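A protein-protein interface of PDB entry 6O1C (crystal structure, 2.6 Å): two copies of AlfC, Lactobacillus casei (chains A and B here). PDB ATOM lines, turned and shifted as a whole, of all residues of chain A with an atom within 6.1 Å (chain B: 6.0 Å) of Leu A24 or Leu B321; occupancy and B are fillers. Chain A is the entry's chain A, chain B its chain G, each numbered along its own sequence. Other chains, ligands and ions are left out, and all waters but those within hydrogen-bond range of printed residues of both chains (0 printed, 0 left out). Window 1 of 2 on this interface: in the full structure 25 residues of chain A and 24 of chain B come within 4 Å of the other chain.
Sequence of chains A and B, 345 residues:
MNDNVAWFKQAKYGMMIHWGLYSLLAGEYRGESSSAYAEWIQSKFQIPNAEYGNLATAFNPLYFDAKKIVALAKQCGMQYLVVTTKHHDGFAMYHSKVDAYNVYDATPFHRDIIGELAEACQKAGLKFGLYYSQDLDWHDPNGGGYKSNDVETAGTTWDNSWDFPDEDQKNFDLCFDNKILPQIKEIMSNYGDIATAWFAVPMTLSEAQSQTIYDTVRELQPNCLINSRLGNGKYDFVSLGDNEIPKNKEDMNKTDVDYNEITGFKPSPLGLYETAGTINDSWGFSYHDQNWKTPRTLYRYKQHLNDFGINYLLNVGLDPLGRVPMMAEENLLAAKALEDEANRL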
ATOM      1  N   GLY A  20      11.042  19.579 -12.537  1.00  0.00           N
ATOM      2  CA  GLY A  20      11.307  20.531 -11.450  1.00  0.00           C
ATOM      3  C   GLY A  20      11.132  21.962 -11.897  1.00  0.00           C
ATOM      4  O   GLY A  20      10.589  22.177 -12.962  1.00  0.00           O
ATOM      5  N   LEU A  21      11.574  22.909 -11.078  1.00  0.00           N
ATOM      6  CA  LEU A  21      11.502  24.347 -11.423  1.00  0.00           C
ATOM      7  C   LEU A  21      12.265  24.572 -12.742  1.00  0.00           C
ATOM      8  O   LEU A  21      11.794  25.402 -13.530  1.00  0.00           O
ATOM      9  CB  LEU A  21      12.056  25.184 -10.257  1.00  0.00           C
ATOM     10  CG  LEU A  21      11.032  25.590  -9.192  1.00  0.00           C
ATOM     11  CD1 LEU A  21      10.128  24.431  -8.824  1.00  0.00           C
ATOM     12  CD2 LEU A  21      11.678  26.169  -7.949  1.00  0.00           C
ATOM     13  N   TYR A  22      13.371  23.856 -12.962  1.00  0.00           N
ATOM     14  CA  TYR A  22      14.234  23.973 -14.178  1.00  0.00           C
ATOM     15  C   TYR A  22      13.368  23.847 -15.442  1.00  0.00           C
ATOM     16  O   TYR A  22      13.591  24.599 -16.418  1.00  0.00           O
ATOM     17  CB  TYR A  22      15.406  22.978 -14.176  1.00  0.00           C
ATOM     18  CG  TYR A  22      15.122  21.564 -13.720  1.00  0.00           C
ATOM     19  CD1 TYR A  22      14.583  20.621 -14.581  1.00  0.00           C
ATOM     20  CD2 TYR A  22      15.431  21.153 -12.431  1.00  0.00           C
ATOM     21  CE1 TYR A  22      14.326  19.323 -14.174  1.00  0.00           C
ATOM     22  CE2 TYR A  22      15.164  19.862 -11.999  1.00  0.00           C
ATOM     23  CZ  TYR A  22      14.625  18.942 -12.881  1.00  0.00           C
ATOM     24  OH  TYR A  22      14.375  17.664 -12.484  1.00  0.00           O
ATOM     25  N   SER A  23      12.372  22.963 -15.402  1.00  0.00           N
ATOM     26  CA  SER A  23      11.433  22.687 -16.522  1.00  0.00           C
ATOM     27  C   SER A  23      10.721  23.967 -16.994  1.00  0.00           C
ATOM     28  O   SER A  23      10.431  24.058 -18.206  1.00  0.00           O
ATOM     29  CB  SER A  23      10.460  21.605 -16.120  1.00  0.00           C
ATOM     30  OG  SER A  23      11.171  20.527 -15.510  1.00  0.00           O
ATOM     31  N   LEU A  24      10.429  24.911 -16.094  1.00  0.00           N
ATOM     32  CA  LEU A  24       9.681  26.137 -16.467  1.00  0.00           C
ATOM     33  C   LEU A  24      10.580  27.022 -17.328  1.00  0.00           C
ATOM     34  O   LEU A  24      10.053  27.627 -18.267  1.00  0.00           O
ATOM     35  CB  LEU A  24       9.182  26.902 -15.239  1.00  0.00           C
ATOM     36  CG  LEU A  24       8.169  26.172 -14.357  1.00  0.00           C
ATOM     37  CD1 LEU A  24       7.556  27.115 -13.336  1.00  0.00           C
ATOM     38  CD2 LEU A  24       7.079  25.486 -15.148  1.00  0.00           C
ATOM     39  N   LEU A  25      11.875  27.092 -17.031  1.00  0.00           N
ATOM     40  CA  LEU A  25      12.827  27.924 -17.817  1.00  0.00           C
ATOM     41  C   LEU A  25      13.105  27.258 -19.169  1.00  0.00           C
ATOM     42  O   LEU A  25      13.490  27.975 -20.109  1.00  0.00           O
ATOM     43  CB  LEU A  25      14.109  28.140 -17.011  1.00  0.00           C
ATOM     44  CG  LEU A  25      14.022  29.219 -15.925  1.00  0.00           C
ATOM     45  CD1 LEU A  25      15.288  29.229 -15.071  1.00  0.00           C
ATOM     46  CD2 LEU A  25      13.786  30.592 -16.533  1.00  0.00           C
ATOM     47  N   ALA A  26      12.969  25.932 -19.247  1.00  0.00           N
ATOM     48  CA  ALA A  26      12.982  25.147 -20.504  1.00  0.00           C
ATOM     49  C   ALA A  26      14.212  25.451 -21.381  1.00  0.00           C
ATOM     50  O   ALA A  26      14.056  25.586 -22.606  1.00  0.00           O
ATOM     51  CB  ALA A  26      11.685  25.420 -21.247  1.00  0.00           C
ATOM     52  N   LEU A  55      10.245  30.630  -9.094  1.00  0.00           N
ATOM     53  CA  LEU A  55       9.618  29.792 -10.151  1.00  0.00           C
ATOM     54  C   LEU A  55       8.522  28.913  -9.537  1.00  0.00           C
ATOM     55  O   LEU A  55       7.546  28.611 -10.259  1.00  0.00           O
ATOM     56  CB  LEU A  55      10.686  28.934 -10.838  1.00  0.00           C
ATOM     57  CG  LEU A  55      11.662  29.711 -11.719  1.00  0.00           C
ATOM     58  CD1 LEU A  55      12.865  28.853 -12.065  1.00  0.00           C
ATOM     59  CD2 LEU A  55      10.993  30.217 -12.970  1.00  0.00           C
ATOM     60  N   ALA A  56       8.668  28.524  -8.261  1.00  0.00           N
ATOM     61  CA  ALA A  56       7.653  27.735  -7.516  1.00  0.00           C
ATOM     62  C   ALA A  56       6.280  28.401  -7.625  1.00  0.00           C
ATOM     63  O   ALA A  56       5.275  27.671  -7.762  1.00  0.00           O
ATOM     64  CB  ALA A  56       8.060  27.560  -6.073  1.00  0.00           C
ATOM     65  N   ALA A  58       5.052  29.981 -10.041  1.00  0.00           N
ATOM     66  CA  ALA A  58       4.526  29.843 -11.420  1.00  0.00           C
ATOM     67  C   ALA A  58       4.302  28.372 -11.783  1.00  0.00           C
ATOM     68  O   ALA A  58       3.831  28.127 -12.885  1.00  0.00           O
ATOM     69  CB  ALA A  58       5.451  30.523 -12.395  1.00  0.00           C
ATOM     70  N   PHE A  59       4.614  27.428 -10.899  1.00  0.00           N
ATOM     71  CA  PHE A  59       4.538  25.968 -11.180  1.00  0.00           C
ATOM     72  C   PHE A  59       3.093  25.485 -10.996  1.00  0.00           C
ATOM     73  O   PHE A  59       2.702  25.225  -9.840  1.00  0.00           O
ATOM     74  CB  PHE A  59       5.508  25.203 -10.274  1.00  0.00           C
ATOM     75  CG  PHE A  59       5.661  23.740 -10.609  1.00  0.00           C
ATOM     76  CD1 PHE A  59       4.782  22.796 -10.107  1.00  0.00           C
ATOM     77  CD2 PHE A  59       6.678  23.310 -11.445  1.00  0.00           C
ATOM     78  CE1 PHE A  59       4.917  21.454 -10.422  1.00  0.00           C
ATOM     79  CE2 PHE A  59       6.800  21.975 -11.777  1.00  0.00           C
ATOM     80  CZ  PHE A  59       5.920  21.050 -11.262  1.00  0.00           C
ATOM     81  N   ASN A  60       2.334  25.346 -12.089  1.00  0.00           N
ATOM     82  CA  ASN A  60       0.902  24.941 -12.069  1.00  0.00           C
ATOM     83  C   ASN A  60       0.617  24.028 -13.264  1.00  0.00           C
ATOM     84  O   ASN A  60      -0.179  24.354 -14.156  1.00  0.00           O
ATOM     85  CB  ASN A  60       0.000  26.175 -12.056  1.00  0.00           C
ATOM     86  CG  ASN A  60      -1.341  25.938 -11.403  1.00  0.00           C
ATOM     87  OD1 ASN A  60      -1.693  24.829 -11.043  1.00  0.00           O
ATOM     88  ND2 ASN A  60      -2.103  26.999 -11.237  1.00  0.00           N
ATOM     89  N   TYR A 287      13.015  23.627 -24.726  1.00  0.00           N
ATOM     90  CA  TYR A 287      12.292  24.013 -25.965  1.00  0.00           C
ATOM     91  C   TYR A 287      13.251  23.880 -27.163  1.00  0.00           C
ATOM     92  O   TYR A 287      12.911  23.293 -28.198  1.00  0.00           O
ATOM     93  CB  TYR A 287      11.823  25.480 -25.932  1.00  0.00           C
ATOM     94  CG  TYR A 287      10.716  25.900 -24.986  1.00  0.00           C
ATOM     95  CD1 TYR A 287       9.576  25.136 -24.802  1.00  0.00           C
ATOM     96  CD2 TYR A 287      10.776  27.121 -24.320  1.00  0.00           C
ATOM     97  CE1 TYR A 287       8.564  25.536 -23.936  1.00  0.00           C
ATOM     98  CE2 TYR A 287       9.773  27.546 -23.460  1.00  0.00           C
ATOM     99  CZ  TYR A 287       8.664  26.745 -23.256  1.00  0.00           C
ATOM    100  OH  TYR A 287       7.696  27.147 -22.384  1.00  0.00           O
ATOM    101  N   ASP A 319       7.205  18.683 -19.485  1.00  0.00           N
ATOM    102  CA  ASP A 319       7.134  20.125 -19.866  1.00  0.00           C
ATOM    103  C   ASP A 319       6.459  20.905 -18.731  1.00  0.00           C
ATOM    104  O   ASP A 319       6.023  20.332 -17.731  1.00  0.00           O
ATOM    105  CB  ASP A 319       6.482  20.299 -21.235  1.00  0.00           C
ATOM    106  CG  ASP A 319       4.957  20.285 -21.244  1.00  0.00           C
ATOM    107  OD1 ASP A 319       4.349  20.016 -20.176  1.00  0.00           O
ATOM    108  OD2 ASP A 319       4.386  20.511 -22.353  1.00  0.00           O
ATOM    109  N   PRO A 320       6.391  22.249 -18.816  1.00  0.00           N
ATOM    110  CA  PRO A 320       5.834  23.050 -17.725  1.00  0.00           C
ATOM    111  C   PRO A 320       4.372  22.722 -17.381  1.00  0.00           C
ATOM    112  O   PRO A 320       4.009  23.015 -16.284  1.00  0.00           O
ATOM    113  CB  PRO A 320       5.941  24.491 -18.244  1.00  0.00           C
ATOM    114  CG  PRO A 320       7.066  24.429 -19.239  1.00  0.00           C
ATOM    115  CD  PRO A 320       6.905  23.077 -19.918  1.00  0.00           C
ATOM    116  N   LEU A 321       3.580  22.145 -18.286  1.00  0.00           N
ATOM    117  CA  LEU A 321       2.181  21.737 -17.985  1.00  0.00           C
ATOM    118  C   LEU A 321       2.127  20.274 -17.520  1.00  0.00           C
ATOM    119  O   LEU A 321       1.012  19.773 -17.306  1.00  0.00           O
ATOM    120  CB  LEU A 321       1.301  21.970 -19.214  1.00  0.00           C
ATOM    121  CG  LEU A 321       0.979  23.438 -19.505  1.00  0.00           C
ATOM    122  CD1 LEU A 321       0.327  23.588 -20.872  1.00  0.00           C
ATOM    123  CD2 LEU A 321       0.096  24.040 -18.414  1.00  0.00           C
ATOM    124  N   TRP B  19       0.045  36.901 -28.063  1.00  0.00           N
ATOM    125  CA  TRP B  19       0.230  36.387 -26.683  1.00  0.00           C
ATOM    126  C   TRP B  19      -1.136  36.185 -26.042  1.00  0.00           C
ATOM    127  O   TRP B  19      -2.018  37.063 -26.200  1.00  0.00           O
ATOM    128  CB  TRP B  19       1.134  37.338 -25.885  1.00  0.00           C
ATOM    129  CG  TRP B  19       1.746  36.724 -24.669  1.00  0.00           C
ATOM    130  CD1 TRP B  19       2.149  35.428 -24.508  1.00  0.00           C
ATOM    131  CD2 TRP B  19       2.046  37.392 -23.429  1.00  0.00           C
ATOM    132  NE1 TRP B  19       2.666  35.244 -23.255  1.00  0.00           N
ATOM    133  CE2 TRP B  19       2.618  36.430 -22.564  1.00  0.00           C
ATOM    134  CE3 TRP B  19       1.884  38.698 -22.957  1.00  0.00           C
ATOM    135  CZ2 TRP B  19       3.027  36.735 -21.263  1.00  0.00           C
ATOM    136  CZ3 TRP B  19       2.284  39.001 -21.671  1.00  0.00           C
ATOM    137  CH2 TRP B  19       2.857  38.031 -20.838  1.00  0.00           C
ATOM    138  N   LEU B  24       0.384  29.103 -23.603  1.00  0.00           N
ATOM    139  CA  LEU B  24       0.730  28.117 -22.547  1.00  0.00           C
ATOM    140  C   LEU B  24       0.705  26.717 -23.149  1.00  0.00           C
ATOM    141  O   LEU B  24       1.555  25.930 -22.755  1.00  0.00           O
ATOM    142  CB  LEU B  24      -0.241  28.207 -21.364  1.00  0.00           C
ATOM    143  CG  LEU B  24      -0.229  29.518 -20.581  1.00  0.00           C
ATOM    144  CD1 LEU B  24      -1.038  29.375 -19.305  1.00  0.00           C
ATOM    145  CD2 LEU B  24       1.189  29.971 -20.272  1.00  0.00           C
ATOM    146  N   ASN B  60       1.147  32.868 -15.423  1.00  0.00           N
ATOM    147  CA  ASN B  60       1.977  33.622 -14.442  1.00  0.00           C
ATOM    148  C   ASN B  60       3.352  33.931 -15.037  1.00  0.00           C
ATOM    149  O   ASN B  60       4.383  33.468 -14.545  1.00  0.00           O
ATOM    150  CB  ASN B  60       2.087  32.822 -13.145  1.00  0.00           C
ATOM    151  CG  ASN B  60       2.290  33.671 -11.907  1.00  0.00           C
ATOM    152  OD1 ASN B  60       2.474  34.889 -11.996  1.00  0.00           O
ATOM    153  ND2 ASN B  60       2.163  33.025 -10.753  1.00  0.00           N
ATOM    154  N   PRO B  61       3.414  34.718 -16.135  1.00  0.00           N
ATOM    155  CA  PRO B  61       4.664  34.944 -16.872  1.00  0.00           C
ATOM    156  C   PRO B  61       5.669  35.815 -16.109  1.00  0.00           C
ATOM    157  O   PRO B  61       5.799  37.010 -16.400  1.00  0.00           O
ATOM    158  CB  PRO B  61       4.178  35.648 -18.141  1.00  0.00           C
ATOM    159  CG  PRO B  61       2.950  36.398 -17.679  1.00  0.00           C
ATOM    160  CD  PRO B  61       2.280  35.454 -16.706  1.00  0.00           C
ATOM    161  N   LEU B  62       6.388  35.167 -15.189  1.00  0.00           N
ATOM    162  CA  LEU B  62       7.349  35.820 -14.270  1.00  0.00           C
ATOM    163  C   LEU B  62       8.341  36.713 -15.006  1.00  0.00           C
ATOM    164  O   LEU B  62       8.796  37.664 -14.388  1.00  0.00           O
ATOM    165  CB  LEU B  62       8.078  34.739 -13.474  1.00  0.00           C
ATOM    166  CG  LEU B  62       7.190  33.967 -12.492  1.00  0.00           C
ATOM    167  CD1 LEU B  62       8.046  33.151 -11.514  1.00  0.00           C
ATOM    168  CD2 LEU B  62       6.228  34.886 -11.727  1.00  0.00           C
ATOM    169  N   TYR B  63       8.702  36.427 -16.254  1.00  0.00           N
ATOM    170  CA  TYR B  63       9.809  37.158 -16.941  1.00  0.00           C
ATOM    171  C   TYR B  63       9.262  38.218 -17.901  1.00  0.00           C
ATOM    172  O   TYR B  63      10.108  38.920 -18.476  1.00  0.00           O
ATOM    173  CB  TYR B  63      10.818  36.182 -17.575  1.00  0.00           C
ATOM    174  CG  TYR B  63      11.708  35.541 -16.550  1.00  0.00           C
ATOM    175  CD1 TYR B  63      11.289  34.421 -15.857  1.00  0.00           C
ATOM    176  CD2 TYR B  63      12.904  36.129 -16.170  1.00  0.00           C
ATOM    177  CE1 TYR B  63      12.071  33.846 -14.864  1.00  0.00           C
ATOM    178  CE2 TYR B  63      13.690  35.583 -15.165  1.00  0.00           C
ATOM    179  CZ  TYR B  63      13.276  34.430 -14.522  1.00  0.00           C
ATOM    180  OH  TYR B  63      14.034  33.888 -13.531  1.00  0.00           O
ATOM    181  N   PHE B  64       7.938  38.384 -18.029  1.00  0.00           N
ATOM    182  CA  PHE B  64       7.347  39.455 -18.879  1.00  0.00           C
ATOM    183  C   PHE B  64       7.928  40.799 -18.461  1.00  0.00           C
ATOM    184  O   PHE B  64       7.959  41.061 -17.280  1.00  0.00           O
ATOM    185  CB  PHE B  64       5.829  39.550 -18.787  1.00  0.00           C
ATOM    186  CG  PHE B  64       5.253  40.654 -19.648  1.00  0.00           C
ATOM    187  CD1 PHE B  64       5.295  40.567 -21.034  1.00  0.00           C
ATOM    188  CD2 PHE B  64       4.695  41.790 -19.081  1.00  0.00           C
ATOM    189  CE1 PHE B  64       4.779  41.579 -21.830  1.00  0.00           C
ATOM    190  CE2 PHE B  64       4.182  42.805 -19.873  1.00  0.00           C
ATOM    191  CZ  PHE B  64       4.234  42.702 -21.250  1.00  0.00           C
ATOM    192  N   ASP B 319       6.534  33.600 -25.102  1.00  0.00           N
ATOM    193  CA  ASP B 319       6.467  32.241 -24.496  1.00  0.00           C
ATOM    194  C   ASP B 319       5.668  32.311 -23.191  1.00  0.00           C
ATOM    195  O   ASP B 319       5.248  33.378 -22.756  1.00  0.00           O
ATOM    196  CB  ASP B 319       7.868  31.644 -24.364  1.00  0.00           C
ATOM    197  CG  ASP B 319       8.654  32.080 -23.128  1.00  0.00           C
ATOM    198  OD1 ASP B 319       8.181  32.980 -22.414  1.00  0.00           O
ATOM    199  OD2 ASP B 319       9.761  31.510 -22.895  1.00  0.00           O
ATOM    200  N   PRO B 320       5.396  31.168 -22.537  1.00  0.00           N
ATOM    201  CA  PRO B 320       4.595  31.154 -21.315  1.00  0.00           C
ATOM    202  C   PRO B 320       5.155  32.010 -20.167  1.00  0.00           C
ATOM    203  O   PRO B 320       4.369  32.380 -19.352  1.00  0.00           O
ATOM    204  CB  PRO B 320       4.591  29.674 -20.898  1.00  0.00           C
ATOM    205  CG  PRO B 320       4.824  28.934 -22.196  1.00  0.00           C
ATOM    206  CD  PRO B 320       5.806  29.812 -22.948  1.00  0.00           C
ATOM    207  N   LEU B 321       6.459  32.299 -20.119  1.00  0.00           N
ATOM    208  CA  LEU B 321       7.053  33.176 -19.078  1.00  0.00           C
ATOM    209  C   LEU B 321       7.112  34.633 -19.560  1.00  0.00           C
ATOM    210  O   LEU B 321       7.650  35.472 -18.819  1.00  0.00           O
ATOM    211  CB  LEU B 321       8.441  32.662 -18.702  1.00  0.00           C
ATOM    212  CG  LEU B 321       8.460  31.384 -17.860  1.00  0.00           C
ATOM    213  CD1 LEU B 321       9.879  30.846 -17.734  1.00  0.00           C
ATOM    214  CD2 LEU B 321       7.852  31.609 -16.482  1.00  0.00           C
ATOM    215  N   GLY B 322       6.555  34.946 -20.731  1.00  0.00           N
ATOM    216  CA  GLY B 322       6.503  36.320 -21.284  1.00  0.00           C
ATOM    217  C   GLY B 322       7.797  36.742 -21.974  1.00  0.00           C
ATOM    218  O   GLY B 322       8.095  37.969 -22.029  1.00  0.00           O
ATOM    219  N   ARG B 323       8.554  35.771 -22.483  1.00  0.00           N
ATOM    220  CA  ARG B 323       9.877  36.008 -23.123  1.00  0.00           C
ATOM    221  C   ARG B 323       9.727  35.974 -24.647  1.00  0.00           C
ATOM    222  O   ARG B 323       8.940  35.148 -25.176  1.00  0.00           O
ATOM    223  CB  ARG B 323      10.892  34.964 -22.653  1.00  0.00           C
ATOM    224  CG  ARG B 323      11.115  35.006 -21.148  1.00  0.00           C
ATOM    225  CD  ARG B 323      12.094  33.981 -20.636  1.00  0.00           C
ATOM    226  NE  ARG B 323      11.723  32.637 -21.052  1.00  0.00           N
ATOM    227  CZ  ARG B 323      12.388  31.539 -20.712  1.00  0.00           C
ATOM    228  NH1 ARG B 323      13.452  31.591 -19.926  1.00  0.00           N
ATOM    229  NH2 ARG B 323      11.976  30.374 -21.171  1.00  0.00           N
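O of Leu A25 sits at hydrogen-bond distance from NH2 of Arg B323, 3.0 Å away.
The backbone carbonyl oxygen (O) of Ala A26 sits at hydrogen-bond distance from the backbone NH (N) of Tyr A287 (3.1 Å). N of Leu A321 lies within hydrogen-bond range of OD1 of Asp A319 (2.9 Å). The backbone NH (N) of Tyr B63 lies within hydrogen-bond range of the backbone carbonyl oxygen (O) of Leu B321, at 2.9 Å. N of Phe B64 lies within hydrogen-bond range of O of Leu B321. The backbone NH (N) of Leu B321 is in hydrogen-bond range of the side-chain carboxylate (OD1) of Asp B319 (2.9 Å). OD2 of Asp B319 lies within salt-bridge range of NE of Arg B323, at 2.9 Å.
Leu B321 touches Leu A24 (CD1 to O, 3.3 Å). Leu A55 touches Leu B62 (CA to CD1, 3.95 Å). CB of Ala A58 touches O of Asn B60, at 3.8 Å. Ala A58 touches Leu B62 (CB to CD1, 3.8 Å). OH of Tyr A287 touches CD of Pro B320, 3.3 Å away. Leu B24 touches Leu A321.
Leu B321 touches just one residue of chain A: Leu A24 (3.3 Å). Printed residues of chain B within 4 Å of Leu A55: Leu B62 (3.95 Å). Printed residues of chain A within 4 Å of Asn B60: Ala A58. Of the printed residues of chain B, Leu A25 touches Arg B323. Printed residues of chain A within 4 Å of Arg B323: Leu A25 (3.0 Å). Printed residues of chain A within 4 Å of Pro B320: Tyr A287. Tyr B63 touches none of the printed residues of chain A. The nearest residue of chain B that does not touch Leu A24 is Arg B323 (4.4 Å). The nearest printed residue of chain A that does not touch Asn B60 is Phe A59 (6.1 Å).
Of the 12 printed residues of chain B, 6 touch a printed residue of chain A. Hydrophobic or aromatic side chains of chain A within 4 Å of the printed part of chain B: Leu A25, Ala A58, Tyr A287 and Leu A321. Among the printed residues, 7 pairs touch across the chains.
Leu A24 touches Leu B321, and with the chains exchanged Leu A321 touches Leu B24. 5 positions are printed for both chains. Of the 7 pairs that touch across the chains among the printed residues, 2 have their exchanged pair printed and touching as well.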
